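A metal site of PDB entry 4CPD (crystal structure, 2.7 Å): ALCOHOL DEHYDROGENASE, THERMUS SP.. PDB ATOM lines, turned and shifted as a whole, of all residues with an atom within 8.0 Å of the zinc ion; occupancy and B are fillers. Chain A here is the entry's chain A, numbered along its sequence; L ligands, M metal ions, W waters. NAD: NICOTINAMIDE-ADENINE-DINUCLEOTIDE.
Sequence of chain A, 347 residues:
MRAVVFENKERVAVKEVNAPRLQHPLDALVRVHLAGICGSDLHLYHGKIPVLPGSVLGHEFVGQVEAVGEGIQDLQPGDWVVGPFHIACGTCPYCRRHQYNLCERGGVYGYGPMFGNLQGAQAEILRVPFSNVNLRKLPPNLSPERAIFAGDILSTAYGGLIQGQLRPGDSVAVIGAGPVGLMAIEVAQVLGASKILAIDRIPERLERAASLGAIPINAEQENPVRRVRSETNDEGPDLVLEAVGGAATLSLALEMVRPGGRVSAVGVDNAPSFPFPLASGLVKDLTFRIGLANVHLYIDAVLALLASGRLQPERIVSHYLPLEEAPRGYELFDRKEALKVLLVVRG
The zinc ion is bound by OD2 of Asp 152, SG of Cys 38, NE2 of His 59 and water W1.
Residues that only touch the zinc ion: Ser 40 (3.7 Å).
Of the 18 residues printed, 4 come within 4 Å of the zinc ion.
Along chain A the residues within 4 Å of the zinc ion span positions 38 to 152.
The nearest printed residue that does not touch the zinc ion is Glu 60 (4.5 Å).
O of Asp 152 is in hydrogen-bond range of OG1 of Thr 156 (2.9 Å).
The side-chain carboxylate (OD1) of Asp 41 sits close to a ring nitrogen (ND1) of His 59 (3.4 Å).
OH of Tyr 111 sits at hydrogen-bond distance from O of Ser 40 (2.8 Å).
N of Cys 38 lies close to OE1 of Glu 60 (3.2 Å).
The side-chain sulfur (SG) of Cys 38 lies close to the backbone NH (N) of Ser 40, 3.4 Å away.
N of Cys 38 lies within hydrogen-bond range of OD2 of Asp 41, at 2.8 Å.
The side-chain hydroxyl (OG) of Ser 40 lies within hydrogen-bond range of an oxygen (O2D) of the ligand, 3.4 Å away.
An oxygen (O2N) of the ligand is in hydrogen-bond range of the backbone NH (N) of Val 180 (3.2 Å).
O1N of the ligand lies within hydrogen-bond range of N of Gly 39, at 3.2 Å.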
ATOM      1  N   GLY A  36     -22.163  21.801  17.912  1.00  0.00           N
ATOM      2  CA  GLY A  36     -21.630  22.542  19.020  1.00  0.00           C
ATOM      3  C   GLY A  36     -22.138  23.975  19.025  1.00  0.00           C
ATOM      4  O   GLY A  36     -22.621  24.491  17.990  1.00  0.00           O
ATOM      5  N   ILE A  37     -22.014  24.580  20.200  1.00  0.00           N
ATOM      6  CA  ILE A  37     -22.066  26.035  20.374  1.00  0.00           C
ATOM      7  C   ILE A  37     -20.670  26.540  20.703  1.00  0.00           C
ATOM      8  O   ILE A  37     -20.060  26.115  21.689  1.00  0.00           O
ATOM      9  CB  ILE A  37     -22.981  26.416  21.519  1.00  0.00           C
ATOM     10  CG1 ILE A  37     -24.400  25.904  21.218  1.00  0.00           C
ATOM     11  CG2 ILE A  37     -22.981  27.930  21.690  1.00  0.00           C
ATOM     12  CD1 ILE A  37     -25.299  25.920  22.435  1.00  0.00           C
ATOM     13  N   CYS A  38     -20.192  27.463  19.850  1.00  0.00           N
ATOM     14  CA  CYS A  38     -18.811  27.966  19.878  1.00  0.00           C
ATOM     15  C   CYS A  38     -18.791  29.376  20.468  1.00  0.00           C
ATOM     16  O   CYS A  38     -19.791  30.103  20.438  1.00  0.00           O
ATOM     17  CB  CYS A  38     -18.245  27.948  18.440  1.00  0.00           C
ATOM     18  SG  CYS A  38     -16.591  28.590  18.230  1.00  0.00           S
ATOM     19  N   GLY A  39     -17.652  29.779  20.990  1.00  0.00           N
ATOM     20  CA  GLY A  39     -17.452  31.155  21.413  1.00  0.00           C
ATOM     21  C   GLY A  39     -17.785  32.150  20.308  1.00  0.00           C
ATOM     22  O   GLY A  39     -18.346  33.212  20.589  1.00  0.00           O
ATOM     23  N   SER A  40     -17.448  31.808  19.057  1.00  0.00           N
ATOM     24  CA  SER A  40     -17.777  32.630  17.897  1.00  0.00           C
ATOM     25  C   SER A  40     -19.282  32.860  17.766  1.00  0.00           C
ATOM     26  O   SER A  40     -19.714  33.896  17.270  1.00  0.00           O
ATOM     27  CB  SER A  40     -17.267  31.996  16.593  1.00  0.00           C
ATOM     28  OG  SER A  40     -15.866  31.782  16.637  1.00  0.00           O
ATOM     29  N   ASP A  41     -20.081  31.885  18.217  1.00  0.00           N
ATOM     30  CA  ASP A  41     -21.512  31.977  18.124  1.00  0.00           C
ATOM     31  C   ASP A  41     -22.008  33.045  19.082  1.00  0.00           C
ATOM     32  O   ASP A  41     -23.077  33.626  18.881  1.00  0.00           O
ATOM     33  CB  ASP A  41     -22.178  30.634  18.433  1.00  0.00           C
ATOM     34  CG  ASP A  41     -21.938  29.584  17.379  1.00  0.00           C
ATOM     35  OD1 ASP A  41     -21.818  29.903  16.166  1.00  0.00           O
ATOM     36  OD2 ASP A  41     -21.911  28.394  17.787  1.00  0.00           O
ATOM     37  N   GLY A  58     -24.751  28.005  13.670  1.00  0.00           N
ATOM     38  CA  GLY A  58     -23.820  26.927  14.027  1.00  0.00           C
ATOM     39  C   GLY A  58     -22.874  26.475  12.913  1.00  0.00           C
ATOM     40  O   GLY A  58     -23.266  26.435  11.737  1.00  0.00           O
ATOM     41  N   HIS A  59     -21.630  26.160  13.287  1.00  0.00           N
ATOM     42  CA  HIS A  59     -20.632  25.696  12.322  1.00  0.00           C
ATOM     43  C   HIS A  59     -19.786  24.533  12.864  1.00  0.00           C
ATOM     44  O   HIS A  59     -18.782  24.151  12.246  1.00  0.00           O
ATOM     45  CB  HIS A  59     -19.728  26.858  11.963  1.00  0.00           C
ATOM     46  CG  HIS A  59     -19.196  27.566  13.163  1.00  0.00           C
ATOM     47  ND1 HIS A  59     -19.798  28.691  13.658  1.00  0.00           N
ATOM     48  CD2 HIS A  59     -18.170  27.268  13.988  1.00  0.00           C
ATOM     49  CE1 HIS A  59     -19.149  29.081  14.739  1.00  0.00           C
ATOM     50  NE2 HIS A  59     -18.166  28.225  14.960  1.00  0.00           N
ATOM     51  N   GLU A  60     -20.180  23.994  14.018  1.00  0.00           N
ATOM     52  CA  GLU A  60     -19.543  22.818  14.566  1.00  0.00           C
ATOM     53  C   GLU A  60     -20.452  21.567  14.423  1.00  0.00           C
ATOM     54  O   GLU A  60     -21.560  21.583  14.950  1.00  0.00           O
ATOM     55  CB  GLU A  60     -19.261  23.042  16.016  1.00  0.00           C
ATOM     56  CG  GLU A  60     -18.168  24.036  16.337  1.00  0.00           C
ATOM     57  CD  GLU A  60     -18.122  24.263  17.837  1.00  0.00           C
ATOM     58  OE1 GLU A  60     -19.052  24.863  18.389  1.00  0.00           O
ATOM     59  OE2 GLU A  60     -17.172  23.817  18.504  1.00  0.00           O
ATOM     60  N   PHE A  85     -15.163  24.281   9.952  1.00  0.00           N
ATOM     61  CA  PHE A  85     -16.190  25.263  10.090  1.00  0.00           C
ATOM     62  C   PHE A  85     -16.226  26.288   8.956  1.00  0.00           C
ATOM     63  O   PHE A  85     -17.164  27.046   8.843  1.00  0.00           O
ATOM     64  CB  PHE A  85     -16.055  25.983  11.424  1.00  0.00           C
ATOM     65  CG  PHE A  85     -14.888  26.927  11.510  1.00  0.00           C
ATOM     66  CD1 PHE A  85     -15.004  28.252  11.089  1.00  0.00           C
ATOM     67  CD2 PHE A  85     -13.699  26.534  12.103  1.00  0.00           C
ATOM     68  CE1 PHE A  85     -13.949  29.147  11.221  1.00  0.00           C
ATOM     69  CE2 PHE A  85     -12.642  27.418  12.226  1.00  0.00           C
ATOM     70  CZ  PHE A  85     -12.766  28.726  11.790  1.00  0.00           C
ATOM     71  N   VAL A 108     -18.277  30.711   6.169  1.00  0.00           N
ATOM     72  CA  VAL A 108     -18.425  30.003   7.425  1.00  0.00           C
ATOM     73  C   VAL A 108     -19.882  29.656   7.598  1.00  0.00           C
ATOM     74  O   VAL A 108     -20.726  30.530   7.511  1.00  0.00           O
ATOM     75  CB  VAL A 108     -18.062  30.886   8.631  1.00  0.00           C
ATOM     76  CG1 VAL A 108     -18.225  30.120   9.936  1.00  0.00           C
ATOM     77  CG2 VAL A 108     -16.652  31.417   8.500  1.00  0.00           C
ATOM     78  N   TYR A 111     -23.041  31.757   9.691  1.00  0.00           N
ATOM     79  CA  TYR A 111     -22.394  32.968  10.172  1.00  0.00           C
ATOM     80  C   TYR A 111     -22.847  34.240   9.405  1.00  0.00           C
ATOM     81  O   TYR A 111     -22.191  35.297   9.448  1.00  0.00           O
ATOM     82  CB  TYR A 111     -20.872  32.777  10.196  1.00  0.00           C
ATOM     83  CG  TYR A 111     -20.244  33.359  11.446  1.00  0.00           C
ATOM     84  CD1 TYR A 111     -20.458  32.771  12.668  1.00  0.00           C
ATOM     85  CD2 TYR A 111     -19.461  34.488  11.382  1.00  0.00           C
ATOM     86  CE1 TYR A 111     -19.889  33.289  13.820  1.00  0.00           C
ATOM     87  CE2 TYR A 111     -18.899  35.034  12.519  1.00  0.00           C
ATOM     88  CZ  TYR A 111     -19.125  34.430  13.747  1.00  0.00           C
ATOM     89  OH  TYR A 111     -18.585  34.955  14.894  1.00  0.00           O
ATOM     90  N   GLY A 151     -13.055  19.790  13.645  1.00  0.00           N
ATOM     91  CA  GLY A 151     -13.597  20.698  12.657  1.00  0.00           C
ATOM     92  C   GLY A 151     -13.433  22.168  12.992  1.00  0.00           C
ATOM     93  O   GLY A 151     -13.509  23.021  12.064  1.00  0.00           O
ATOM     94  N   ASP A 152     -13.184  22.478  14.283  1.00  0.00           N
ATOM     95  CA  ASP A 152     -13.100  23.896  14.689  1.00  0.00           C
ATOM     96  C   ASP A 152     -12.102  24.136  15.793  1.00  0.00           C
ATOM     97  O   ASP A 152     -10.947  24.388  15.509  1.00  0.00           O
ATOM     98  CB  ASP A 152     -14.517  24.416  14.996  1.00  0.00           C
ATOM     99  CG  ASP A 152     -14.546  25.826  15.428  1.00  0.00           C
ATOM    100  OD1 ASP A 152     -13.480  26.461  15.587  1.00  0.00           O
ATOM    101  OD2 ASP A 152     -15.667  26.312  15.649  1.00  0.00           O
ATOM    102  N   ILE A 153     -12.508  24.053  17.053  1.00  0.00           N
ATOM    103  CA  ILE A 153     -11.664  24.605  18.118  1.00  0.00           C
ATOM    104  C   ILE A 153     -10.303  23.886  18.394  1.00  0.00           C
ATOM    105  O   ILE A 153      -9.342  24.522  18.795  1.00  0.00           O
ATOM    106  CB  ILE A 153     -12.423  24.781  19.425  1.00  0.00           C
ATOM    107  CG1 ILE A 153     -12.965  23.444  19.916  1.00  0.00           C
ATOM    108  CG2 ILE A 153     -13.570  25.766  19.262  1.00  0.00           C
ATOM    109  CD1 ILE A 153     -13.316  23.516  21.390  1.00  0.00           C
ATOM    110  N   THR A 156      -7.997  24.800  15.453  1.00  0.00           N
ATOM    111  CA  THR A 156      -7.659  26.201  15.631  1.00  0.00           C
ATOM    112  C   THR A 156      -6.453  26.343  16.567  1.00  0.00           C
ATOM    113  O   THR A 156      -5.478  27.017  16.243  1.00  0.00           O
ATOM    114  CB  THR A 156      -8.885  26.989  16.160  1.00  0.00           C
ATOM    115  OG1 THR A 156      -9.884  27.041  15.145  1.00  0.00           O
ATOM    116  CG2 THR A 156      -8.545  28.379  16.507  1.00  0.00           C
ATOM    117  N   VAL A 180     -10.939  27.003  23.529  1.00  0.00           N
ATOM    118  CA  VAL A 180      -9.806  27.048  22.595  1.00  0.00           C
ATOM    119  C   VAL A 180      -8.505  26.977  23.350  1.00  0.00           C
ATOM    120  O   VAL A 180      -7.656  26.173  23.011  1.00  0.00           O
ATOM    121  CB  VAL A 180      -9.847  28.304  21.701  1.00  0.00           C
ATOM    122  CG1 VAL A 180      -8.560  28.467  20.916  1.00  0.00           C
ATOM    123  CG2 VAL A 180     -11.049  28.219  20.751  1.00  0.00           C
ATOM    124  N   LYS A 340     -18.501  23.965  27.722  1.00  0.00           N
ATOM    125  CA  LYS A 340     -18.742  23.646  26.337  1.00  0.00           C
ATOM    126  C   LYS A 340     -20.051  22.897  26.225  1.00  0.00           C
ATOM    127  O   LYS A 340     -20.273  21.914  26.932  1.00  0.00           O
ATOM    128  CB  LYS A 340     -17.618  22.781  25.774  1.00  0.00           C
ATOM    129  CG  LYS A 340     -17.757  22.465  24.284  1.00  0.00           C
ATOM    130  CD  LYS A 340     -17.627  23.706  23.400  1.00  0.00           C
ATOM    131  CE  LYS A 340     -17.655  23.357  21.924  1.00  0.00           C
ATOM    132  NZ  LYS A 340     -17.331  24.517  21.070  1.00  0.00           N
HETATM  133  PA  NAD L   1     -14.948  31.828  25.273  1.00  0.00           P
HETATM  134  O1A NAD L   1     -15.861  30.694  25.712  1.00  0.00           O
HETATM  135  O2A NAD L   1     -15.478  33.262  25.282  1.00  0.00           O
HETATM  136  O5B NAD L   1     -13.529  31.840  26.047  1.00  0.00           O
HETATM  137  C5B NAD L   1     -12.860  33.063  26.363  1.00  0.00           C
HETATM  138  C4B NAD L   1     -12.064  32.912  27.644  1.00  0.00           C
HETATM  139  O4B NAD L   1     -11.156  34.017  27.790  1.00  0.00           O
HETATM  140  C3B NAD L   1     -12.976  32.890  28.872  1.00  0.00           C
HETATM  141  O3B NAD L   1     -12.616  31.889  29.837  1.00  0.00           O
HETATM  142  C2B NAD L   1     -12.763  34.253  29.495  1.00  0.00           C
HETATM  143  O2B NAD L   1     -12.967  34.233  30.906  1.00  0.00           O
HETATM  144  C1B NAD L   1     -11.332  34.526  29.104  1.00  0.00           C
HETATM  145  N9A NAD L   1     -11.068  35.974  29.150  1.00  0.00           N
HETATM  146  C8A NAD L   1     -11.897  36.919  28.676  1.00  0.00           C
HETATM  147  N7A NAD L   1     -11.340  38.141  28.891  1.00  0.00           N
HETATM  148  C5A NAD L   1     -10.158  37.960  29.509  1.00  0.00           C
HETATM  149  C6A NAD L   1      -9.063  38.821  30.008  1.00  0.00           C
HETATM  150  N6A NAD L   1      -9.173  40.150  29.857  1.00  0.00           N
HETATM  151  N1A NAD L   1      -7.978  38.253  30.600  1.00  0.00           N
HETATM  152  C2A NAD L   1      -7.871  36.920  30.732  1.00  0.00           C
HETATM  153  N3A NAD L   1      -8.839  36.074  30.297  1.00  0.00           N
HETATM  154  C4A NAD L   1      -9.974  36.515  29.692  1.00  0.00           C
HETATM  155  O3  NAD L   1     -14.447  31.565  23.748  1.00  0.00           O
HETATM  156  PN  NAD L   1     -13.754  30.244  23.122  1.00  0.00           P
HETATM  157  O1N NAD L   1     -14.907  29.372  22.680  1.00  0.00           O
HETATM  158  O2N NAD L   1     -12.592  29.748  23.986  1.00  0.00           O
HETATM  159  O5D NAD L   1     -13.031  30.893  21.830  1.00  0.00           O
HETATM  160  C5D NAD L   1     -11.773  31.573  22.042  1.00  0.00           C
HETATM  161  C4D NAD L   1     -11.515  32.775  21.150  1.00  0.00           C
HETATM  162  O4D NAD L   1     -10.965  32.304  19.915  1.00  0.00           O
HETATM  163  C3D NAD L   1     -12.759  33.587  20.797  1.00  0.00           C
HETATM  164  O3D NAD L   1     -12.386  34.965  20.657  1.00  0.00           O
HETATM  165  C2D NAD L   1     -13.233  32.971  19.479  1.00  0.00           C
HETATM  166  O2D NAD L   1     -14.087  33.803  18.659  1.00  0.00           O
HETATM  167  C1D NAD L   1     -11.879  32.659  18.843  1.00  0.00           C
HETATM  168  N1N NAD L   1     -11.923  31.618  17.805  1.00  0.00           N
HETATM  169  C2N NAD L   1     -11.160  31.878  16.732  1.00  0.00           C
HETATM  170  C3N NAD L   1     -11.080  31.017  15.657  1.00  0.00           C
HETATM  171  C7N NAD L   1     -10.173  31.431  14.538  1.00  0.00           C
HETATM  172  O7N NAD L   1     -10.369  31.053  13.388  1.00  0.00           O
HETATM  173  N7N NAD L   1      -9.123  32.213  14.854  1.00  0.00           N
HETATM  174  C4N NAD L   1     -11.819  29.815  15.687  1.00  0.00           C
HETATM  175  C5N NAD L   1     -12.609  29.548  16.809  1.00  0.00           C
HETATM  176  C6N NAD L   1     -12.652  30.471  17.872  1.00  0.00           C
HETATM  177 ZN    ZN M   1     -16.196  28.115  16.075  1.00  0.00          ZN
HETATM  178  O   HOH W   1     -14.784  29.754  14.866  1.00  0.00           O
